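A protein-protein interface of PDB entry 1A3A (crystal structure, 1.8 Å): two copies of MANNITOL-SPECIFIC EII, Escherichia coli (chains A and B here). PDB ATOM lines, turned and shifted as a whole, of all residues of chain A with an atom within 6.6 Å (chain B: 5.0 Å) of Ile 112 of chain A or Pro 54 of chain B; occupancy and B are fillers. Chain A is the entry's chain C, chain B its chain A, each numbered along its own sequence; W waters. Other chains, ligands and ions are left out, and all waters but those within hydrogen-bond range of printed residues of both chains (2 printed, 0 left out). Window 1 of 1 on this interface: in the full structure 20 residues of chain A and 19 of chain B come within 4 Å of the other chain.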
ATOM      1  N   HIS A  65       1.143  11.556  17.174  1.00  0.00           N
ATOM      2  CA  HIS A  65      -0.043  11.899  17.983  1.00  0.00           C
ATOM      3  C   HIS A  65      -1.280  11.519  17.186  1.00  0.00           C
ATOM      4  O   HIS A  65      -1.176  11.112  16.027  1.00  0.00           O
ATOM      5  CB  HIS A  65      -0.035  13.393  18.338  1.00  0.00           C
ATOM      6  CG  HIS A  65       0.036  14.373  17.211  1.00  0.00           C
ATOM      7  ND1 HIS A  65       1.244  14.769  16.666  1.00  0.00           N
ATOM      8  CD2 HIS A  65      -0.914  15.072  16.549  1.00  0.00           C
ATOM      9  CE1 HIS A  65       1.022  15.650  15.693  1.00  0.00           C
ATOM     10  NE2 HIS A  65      -0.276  15.867  15.611  1.00  0.00           N
ATOM     11  N   VAL A  68      -7.320  14.584  14.714  1.00  0.00           N
ATOM     12  CA  VAL A  68      -8.272  15.471  15.376  1.00  0.00           C
ATOM     13  C   VAL A  68      -9.579  14.748  15.677  1.00  0.00           C
ATOM     14  O   VAL A  68     -10.255  15.020  16.668  1.00  0.00           O
ATOM     15  CB  VAL A  68      -8.579  16.735  14.558  1.00  0.00           C
ATOM     16  CG1 VAL A  68      -7.350  17.639  14.463  1.00  0.00           C
ATOM     17  CG2 VAL A  68      -9.090  16.380  13.172  1.00  0.00           C
ATOM     18  N   ILE A 104       2.585  11.566  21.902  1.00  0.00           N
ATOM     19  CA  ILE A 104       1.930  12.687  22.570  1.00  0.00           C
ATOM     20  C   ILE A 104       0.420  12.470  22.629  1.00  0.00           C
ATOM     21  O   ILE A 104      -0.154  12.066  21.631  1.00  0.00           O
ATOM     22  CB  ILE A 104       2.120  13.999  21.775  1.00  0.00           C
ATOM     23  CG1 ILE A 104       3.594  14.374  21.587  1.00  0.00           C
ATOM     24  CG2 ILE A 104       1.376  15.182  22.393  1.00  0.00           C
ATOM     25  CD1 ILE A 104       4.393  14.517  22.853  1.00  0.00           C
ATOM     26  N   ALA A 106      -2.440  15.100  24.079  1.00  0.00           N
ATOM     27  CA  ALA A 106      -2.925  16.225  24.888  1.00  0.00           C
ATOM     28  C   ALA A 106      -4.448  16.229  24.799  1.00  0.00           C
ATOM     29  O   ALA A 106      -5.010  15.780  23.805  1.00  0.00           O
ATOM     30  CB  ALA A 106      -2.376  17.533  24.360  1.00  0.00           C
ATOM     31  N   ASN A 108      -8.209  17.648  24.296  1.00  0.00           N
ATOM     32  CA  ASN A 108      -8.824  18.603  23.393  1.00  0.00           C
ATOM     33  C   ASN A 108      -7.971  18.967  22.190  1.00  0.00           C
ATOM     34  O   ASN A 108      -7.941  20.115  21.755  1.00  0.00           O
ATOM     35  CB  ASN A 108      -9.137  19.862  24.232  1.00  0.00           C
ATOM     36  CG  ASN A 108     -10.381  19.633  25.071  1.00  0.00           C
ATOM     37  OD1 ASN A 108     -11.118  18.673  24.831  1.00  0.00           O
ATOM     38  ND2 ASN A 108     -10.637  20.484  26.049  1.00  0.00           N
ATOM     39  N   ASN A 109      -7.296  17.986  21.602  1.00  0.00           N
ATOM     40  CA  ASN A 109      -6.466  18.148  20.428  1.00  0.00           C
ATOM     41  C   ASN A 109      -5.383  19.211  20.589  1.00  0.00           C
ATOM     42  O   ASN A 109      -4.895  19.709  19.552  1.00  0.00           O
ATOM     43  CB  ASN A 109      -7.334  18.508  19.211  1.00  0.00           C
ATOM     44  CG  ASN A 109      -8.165  17.355  18.691  1.00  0.00           C
ATOM     45  OD1 ASN A 109      -7.856  16.188  18.931  1.00  0.00           O
ATOM     46  ND2 ASN A 109      -9.242  17.651  17.972  1.00  0.00           N
ATOM     47  N   GLU A 110      -4.900  19.452  21.801  1.00  0.00           N
ATOM     48  CA  GLU A 110      -3.899  20.485  22.036  1.00  0.00           C
ATOM     49  C   GLU A 110      -2.484  19.974  21.976  1.00  0.00           C
ATOM     50  O   GLU A 110      -1.582  20.411  22.693  1.00  0.00           O
ATOM     51  CB  GLU A 110      -4.192  21.160  23.397  1.00  0.00           C
ATOM     52  CG  GLU A 110      -5.466  21.997  23.211  1.00  0.00           C
ATOM     53  CD  GLU A 110      -5.983  22.569  24.509  1.00  0.00           C
ATOM     54  OE1 GLU A 110      -5.434  22.256  25.580  1.00  0.00           O
ATOM     55  OE2 GLU A 110      -6.944  23.384  24.432  1.00  0.00           O
ATOM     56  N   HIS A 111      -2.272  19.011  21.063  1.00  0.00           N
ATOM     57  CA  HIS A 111      -0.963  18.384  20.914  1.00  0.00           C
ATOM     58  C   HIS A 111       0.144  19.384  20.672  1.00  0.00           C
ATOM     59  O   HIS A 111       1.252  19.215  21.180  1.00  0.00           O
ATOM     60  CB  HIS A 111      -1.052  17.363  19.780  1.00  0.00           C
ATOM     61  CG  HIS A 111      -2.193  16.398  19.888  1.00  0.00           C
ATOM     62  ND1 HIS A 111      -2.387  15.586  20.982  1.00  0.00           N
ATOM     63  CD2 HIS A 111      -3.193  16.127  19.025  1.00  0.00           C
ATOM     64  CE1 HIS A 111      -3.465  14.843  20.782  1.00  0.00           C
ATOM     65  NE2 HIS A 111      -3.978  15.154  19.601  1.00  0.00           N
ATOM     66  N   ILE A 112      -0.090  20.466  19.923  1.00  0.00           N
ATOM     67  CA  ILE A 112       0.938  21.463  19.665  1.00  0.00           C
ATOM     68  C   ILE A 112       1.469  22.101  20.934  1.00  0.00           C
ATOM     69  O   ILE A 112       2.614  22.533  21.006  1.00  0.00           O
ATOM     70  CB  ILE A 112       0.435  22.549  18.684  1.00  0.00           C
ATOM     71  CG1 ILE A 112       1.611  23.380  18.175  1.00  0.00           C
ATOM     72  CG2 ILE A 112      -0.639  23.417  19.341  1.00  0.00           C
ATOM     73  CD1 ILE A 112       1.242  24.361  17.064  1.00  0.00           C
ATOM     74  N   GLN A 113       0.674  22.177  22.021  1.00  0.00           N
ATOM     75  CA  GLN A 113       1.152  22.756  23.257  1.00  0.00           C
ATOM     76  C   GLN A 113       2.219  21.868  23.906  1.00  0.00           C
ATOM     77  O   GLN A 113       3.194  22.350  24.467  1.00  0.00           O
ATOM     78  CB  GLN A 113      -0.027  23.011  24.201  1.00  0.00           C
ATOM     79  CG  GLN A 113      -1.042  23.981  23.599  1.00  0.00           C
ATOM     80  CD  GLN A 113      -2.138  24.362  24.572  1.00  0.00           C
ATOM     81  OE1 GLN A 113      -1.959  24.199  25.780  1.00  0.00           O
ATOM     82  NE2 GLN A 113      -3.252  24.876  24.059  1.00  0.00           N
ATOM     83  N   VAL A 114       2.000  20.565  23.829  1.00  0.00           N
ATOM     84  CA  VAL A 114       3.005  19.615  24.331  1.00  0.00           C
ATOM     85  C   VAL A 114       4.211  19.639  23.397  1.00  0.00           C
ATOM     86  O   VAL A 114       5.351  19.650  23.881  1.00  0.00           O
ATOM     87  CB  VAL A 114       2.411  18.201  24.410  1.00  0.00           C
ATOM     88  CG1 VAL A 114       3.465  17.202  24.867  1.00  0.00           C
ATOM     89  CG2 VAL A 114       1.195  18.211  25.331  1.00  0.00           C
ATOM     90  N   ILE A 115       3.997  19.645  22.081  1.00  0.00           N
ATOM     91  CA  ILE A 115       5.148  19.697  21.162  1.00  0.00           C
ATOM     92  C   ILE A 115       6.001  20.923  21.425  1.00  0.00           C
ATOM     93  O   ILE A 115       7.239  20.903  21.507  1.00  0.00           O
ATOM     94  CB  ILE A 115       4.700  19.651  19.692  1.00  0.00           C
ATOM     95  CG1 ILE A 115       4.123  18.287  19.305  1.00  0.00           C
ATOM     96  CG2 ILE A 115       5.816  20.000  18.703  1.00  0.00           C
ATOM     97  CD1 ILE A 115       3.294  18.387  18.025  1.00  0.00           C
ATOM     98  N   THR A 116       5.356  22.080  21.585  1.00  0.00           N
ATOM     99  CA  THR A 116       6.019  23.341  21.853  1.00  0.00           C
ATOM    100  C   THR A 116       6.800  23.305  23.158  1.00  0.00           C
ATOM    101  O   THR A 116       7.913  23.832  23.195  1.00  0.00           O
ATOM    102  CB  THR A 116       5.013  24.517  21.889  1.00  0.00           C
ATOM    103  OG1 THR A 116       4.344  24.495  20.632  1.00  0.00           O
ATOM    104  CG2 THR A 116       5.759  25.839  22.031  1.00  0.00           C
ATOM    105  N   SER A 117       6.232  22.701  24.209  1.00  0.00           N
ATOM    106  CA  SER A 117       6.973  22.582  25.458  1.00  0.00           C
ATOM    107  C   SER A 117       8.266  21.785  25.194  1.00  0.00           C
ATOM    108  O   SER A 117       9.376  22.190  25.566  1.00  0.00           O
ATOM    109  CB  SER A 117       6.137  21.871  26.526  1.00  0.00           C
ATOM    110  OG  SER A 117       6.937  21.709  27.697  1.00  0.00           O
ATOM    111  N   LYS B  21     -12.022  30.373  12.843  1.00  0.00           N
ATOM    112  CA  LYS B  21     -10.568  30.247  12.722  1.00  0.00           C
ATOM    113  C   LYS B  21     -10.161  30.028  11.265  1.00  0.00           C
ATOM    114  O   LYS B  21      -9.108  30.538  10.864  1.00  0.00           O
ATOM    115  CB  LYS B  21     -10.022  29.140  13.624  1.00  0.00           C
ATOM    116  CG  LYS B  21     -10.474  27.717  13.287  1.00  0.00           C
ATOM    117  CD  LYS B  21      -9.830  26.766  14.282  1.00  0.00           C
ATOM    118  CE  LYS B  21      -9.616  25.348  13.819  1.00  0.00           C
ATOM    119  NZ  LYS B  21      -8.704  24.650  14.794  1.00  0.00           N
ATOM    120  N   ARG B  49      -2.698  22.171   7.510  1.00  0.00           N
ATOM    121  CA  ARG B  49      -1.953  21.934   8.752  1.00  0.00           C
ATOM    122  C   ARG B  49      -2.921  21.981   9.924  1.00  0.00           C
ATOM    123  O   ARG B  49      -2.868  21.146  10.842  1.00  0.00           O
ATOM    124  CB  ARG B  49      -0.807  22.922   8.917  1.00  0.00           C
ATOM    125  CG  ARG B  49      -0.250  23.097  10.328  1.00  0.00           C
ATOM    126  CD  ARG B  49       0.574  21.860  10.695  1.00  0.00           C
ATOM    127  NE  ARG B  49       1.885  21.893  10.060  1.00  0.00           N
ATOM    128  CZ  ARG B  49       2.809  20.942  10.167  1.00  0.00           C
ATOM    129  NH1 ARG B  49       2.551  19.855  10.892  1.00  0.00           N
ATOM    130  NH2 ARG B  49       3.980  21.090   9.565  1.00  0.00           N
ATOM    131  N   GLU B  50      -3.857  22.939   9.899  1.00  0.00           N
ATOM    132  CA  GLU B  50      -4.811  23.079  10.988  1.00  0.00           C
ATOM    133  C   GLU B  50      -5.679  21.852  11.208  1.00  0.00           C
ATOM    134  O   GLU B  50      -6.074  21.588  12.349  1.00  0.00           O
ATOM    135  CB  GLU B  50      -5.697  24.312  10.757  1.00  0.00           C
ATOM    136  CG  GLU B  50      -6.436  24.737  12.014  1.00  0.00           C
ATOM    137  CD  GLU B  50      -5.510  25.322  13.071  1.00  0.00           C
ATOM    138  OE1 GLU B  50      -4.462  25.900  12.720  1.00  0.00           O
ATOM    139  OE2 GLU B  50      -5.905  25.284  14.256  1.00  0.00           O
ATOM    140  N   LEU B  52      -4.577  18.817  10.771  1.00  0.00           N
ATOM    141  CA  LEU B  52      -3.653  17.759  11.171  1.00  0.00           C
ATOM    142  C   LEU B  52      -3.262  17.911  12.629  1.00  0.00           C
ATOM    143  O   LEU B  52      -3.194  16.950  13.394  1.00  0.00           O
ATOM    144  CB  LEU B  52      -2.398  17.839  10.288  1.00  0.00           C
ATOM    145  CG  LEU B  52      -2.652  17.635   8.785  1.00  0.00           C
ATOM    146  CD1 LEU B  52      -1.365  17.757   7.989  1.00  0.00           C
ATOM    147  CD2 LEU B  52      -3.308  16.285   8.530  1.00  0.00           C
ATOM    148  N   THR B  53      -2.881  19.132  12.985  1.00  0.00           N
ATOM    149  CA  THR B  53      -2.416  19.484  14.324  1.00  0.00           C
ATOM    150  C   THR B  53      -2.843  20.930  14.566  1.00  0.00           C
ATOM    151  O   THR B  53      -2.178  21.853  14.083  1.00  0.00           O
ATOM    152  CB  THR B  53      -0.892  19.355  14.442  1.00  0.00           C
ATOM    153  OG1 THR B  53      -0.441  18.035  14.066  1.00  0.00           O
ATOM    154  CG2 THR B  53      -0.388  19.593  15.868  1.00  0.00           C
ATOM    155  N   PRO B  54      -3.972  21.130  15.241  1.00  0.00           N
ATOM    156  CA  PRO B  54      -4.484  22.467  15.509  1.00  0.00           C
ATOM    157  C   PRO B  54      -3.441  23.383  16.129  1.00  0.00           C
ATOM    158  O   PRO B  54      -2.652  22.943  16.969  1.00  0.00           O
ATOM    159  CB  PRO B  54      -5.625  22.213  16.475  1.00  0.00           C
ATOM    160  CG  PRO B  54      -6.095  20.832  16.153  1.00  0.00           C
ATOM    161  CD  PRO B  54      -4.825  20.065  15.816  1.00  0.00           C
ATOM    162  N   THR B  55      -3.422  24.668  15.791  1.00  0.00           N
ATOM    163  CA  THR B  55      -2.375  25.564  16.194  1.00  0.00           C
ATOM    164  C   THR B  55      -2.686  26.572  17.293  1.00  0.00           C
ATOM    165  O   THR B  55      -1.982  27.550  17.469  1.00  0.00           O
ATOM    166  CB  THR B  55      -1.823  26.318  14.948  1.00  0.00           C
ATOM    167  OG1 THR B  55      -2.830  27.197  14.465  1.00  0.00           O
ATOM    168  CG2 THR B  55      -1.395  25.327  13.885  1.00  0.00           C
ATOM    169  N   TYR B  56      -3.670  26.246  18.126  1.00  0.00           N
ATOM    170  CA  TYR B  56      -3.988  27.097  19.283  1.00  0.00           C
ATOM    171  C   TYR B  56      -3.012  26.758  20.403  1.00  0.00           C
ATOM    172  O   TYR B  56      -2.942  25.625  20.896  1.00  0.00           O
ATOM    173  CB  TYR B  56      -5.443  26.830  19.635  1.00  0.00           C
ATOM    174  CG  TYR B  56      -5.804  27.382  21.002  1.00  0.00           C
ATOM    175  CD1 TYR B  56      -5.794  28.745  21.237  1.00  0.00           C
ATOM    176  CD2 TYR B  56      -6.133  26.504  22.019  1.00  0.00           C
ATOM    177  CE1 TYR B  56      -6.123  29.240  22.495  1.00  0.00           C
ATOM    178  CE2 TYR B  56      -6.452  26.988  23.271  1.00  0.00           C
ATOM    179  CZ  TYR B  56      -6.456  28.344  23.485  1.00  0.00           C
ATOM    180  OH  TYR B  56      -6.788  28.800  24.740  1.00  0.00           O
ATOM    181  N   LEU B  57      -2.192  27.700  20.818  1.00  0.00           N
ATOM    182  CA  LEU B  57      -1.139  27.496  21.794  1.00  0.00           C
ATOM    183  C   LEU B  57      -1.595  27.697  23.240  1.00  0.00           C
ATOM    184  O   LEU B  57      -0.865  27.384  24.189  1.00  0.00           O
ATOM    185  CB  LEU B  57       0.015  28.478  21.549  1.00  0.00           C
ATOM    186  CG  LEU B  57       0.898  28.259  20.308  1.00  0.00           C
ATOM    187  CD1 LEU B  57       2.077  29.226  20.345  1.00  0.00           C
ATOM    188  CD2 LEU B  57       1.380  26.812  20.251  1.00  0.00           C
ATOM    189  N   VAL B  63      -0.833  29.904  16.134  1.00  0.00           N
ATOM    190  CA  VAL B  63       0.302  30.100  15.203  1.00  0.00           C
ATOM    191  C   VAL B  63       0.165  29.247  13.959  1.00  0.00           C
ATOM    192  O   VAL B  63       0.908  28.285  13.712  1.00  0.00           O
ATOM    193  CB  VAL B  63       1.642  29.747  15.913  1.00  0.00           C
ATOM    194  CG1 VAL B  63       2.052  30.796  16.937  1.00  0.00           C
ATOM    195  CG2 VAL B  63       1.551  28.423  16.670  1.00  0.00           C
ATOM    196  N   HIS B  65       0.482  27.603  10.503  1.00  0.00           N
ATOM    197  CA  HIS B  65       1.684  27.505   9.652  1.00  0.00           C
ATOM    198  C   HIS B  65       1.386  26.480   8.565  1.00  0.00           C
ATOM    199  O   HIS B  65       0.331  25.847   8.544  1.00  0.00           O
ATOM    200  CB  HIS B  65       2.905  27.201  10.498  1.00  0.00           C
ATOM    201  CG  HIS B  65       2.785  25.997  11.385  1.00  0.00           C
ATOM    202  ND1 HIS B  65       2.115  26.059  12.595  1.00  0.00           N
ATOM    203  CD2 HIS B  65       3.205  24.717  11.240  1.00  0.00           C
ATOM    204  CE1 HIS B  65       2.149  24.866  13.166  1.00  0.00           C
ATOM    205  NE2 HIS B  65       2.806  24.035  12.375  1.00  0.00           N
ATOM    206  N   ILE B 115       8.100  29.404  16.391  1.00  0.00           N
ATOM    207  CA  ILE B 115       7.193  29.257  17.532  1.00  0.00           C
ATOM    208  C   ILE B 115       7.946  29.400  18.843  1.00  0.00           C
ATOM    209  O   ILE B 115       7.461  30.049  19.789  1.00  0.00           O
ATOM    210  CB  ILE B 115       6.401  27.943  17.430  1.00  0.00           C
ATOM    211  CG1 ILE B 115       5.436  27.958  16.244  1.00  0.00           C
ATOM    212  CG2 ILE B 115       5.640  27.653  18.722  1.00  0.00           C
ATOM    213  CD1 ILE B 115       4.848  26.597  15.908  1.00  0.00           C
HETATM  214  O   HOH W   1      -5.803  14.924  12.277  1.00  0.00           O
HETATM  215  O   HOH W   2      -2.631  20.870  18.573  1.00  0.00           O
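OG1 of Thr 53 of chain B sits at hydrogen-bond distance from NE2 of His 65 of chain A (2.7 Å). O of Tyr 56 of chain B sits at hydrogen-bond distance from NE2 of Gln 113 of chain A, 3.3 Å away. NE2 of Gln 113 of chain A sits close to O of Leu 57 of chain B (3.5 Å).
The side-chain carboxylate (OE1) of Glu 50 of chain B sits at hydrogen-bond distance from the side-chain hydroxyl (OG1) of Thr 55 of chain B (2.7 Å). N of Val 63 of chain B sits at hydrogen-bond distance from O of Thr 55 of chain B (2.9 Å). ND2 of Asn 109 of chain A sits at hydrogen-bond distance from O of Val 68 of chain A (3.1 Å). OG1 of Thr 116 of chain A is in hydrogen-bond range of O of Ile 112 of chain A, at 2.6 Å.
Among the printed residues, merely in contact across the chains: Ile 112 of chain A with Pro 54 of chain B (3.1 Å), Ile 112 of chain A with Tyr 56 of chain B (3.5 Å), Asn 109 of chain A with Pro 54 of chain B (3.8 Å), Val 68 of chain A with Pro 54 of chain B (3.8 Å), Thr 116 of chain A with Ile 115 of chain B (3.8 Å), Thr 116 of chain A with Leu 57 of chain B (3.8 Å), Glu 110 of chain A with Tyr 56 of chain B (3.8 Å), His 65 of chain A with Leu 52 of chain B (3.8 Å) and Ile 112 of chain A with Thr 55 of chain B (3.9 Å).
Printed residues of chain B within 4 Å of His 65 of chain A: Leu 52 and Thr 53. Ala 106 of chain A touches none of the printed residues of chain B. Of the printed residues of chain B, Ile 112 of chain A touches Pro 54, Thr 55 and Tyr 56. Of the printed residues of chain B, Gln 113 of chain A touches Tyr 56 (3.3 Å) and Leu 57 (3.3 Å). Glu 50 of chain B touches none of the printed residues of chain A. Of chain A, only Val 68 (3.8 Å), Asn 109 (3.8 Å) and Ile 112 (3.1 Å) come within 4 Å of Pro 54 of chain B. The nearest printed residue of chain B that does not touch Ile 112 of chain A is Leu 57 of chain B (4.02 Å).
Printed residues of chain B that touch a printed residue of chain A: Leu 52, Thr 53, Pro 54, Thr 55, Tyr 56, Leu 57 and Ile 115. Hydrophobic or aromatic side chains of chain B that line the printed part of chain A: Pro 54, Tyr 56, Leu 57 and Ile 115. Along chain B the printed residues that touch a printed residue of chain A span positions 52 to 115. Of the 14 printed residues of chain A, 7 touch a printed residue of chain B. Hydrophobic or aromatic side chains of chain A within 4 Å of the printed part of chain B: His 65, Val 68 and Ile 112.
Positions printed for both chains: 65 and 115. Of the 12 pairs that touch across the chains among the printed residues, none has its exchanged pair printed and touching as well.
Water W2 lies within hydrogen-bond range of O of Pro 54 of chain B, O of Asn 109 of chain A, N of Ile 112 of chain A and N of His 111 of chain A. Water W1 lies within hydrogen-bond range of N of Val 68 of chain A (2.9 Å) and O of Leu 52 of chain B (3.5 Å).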
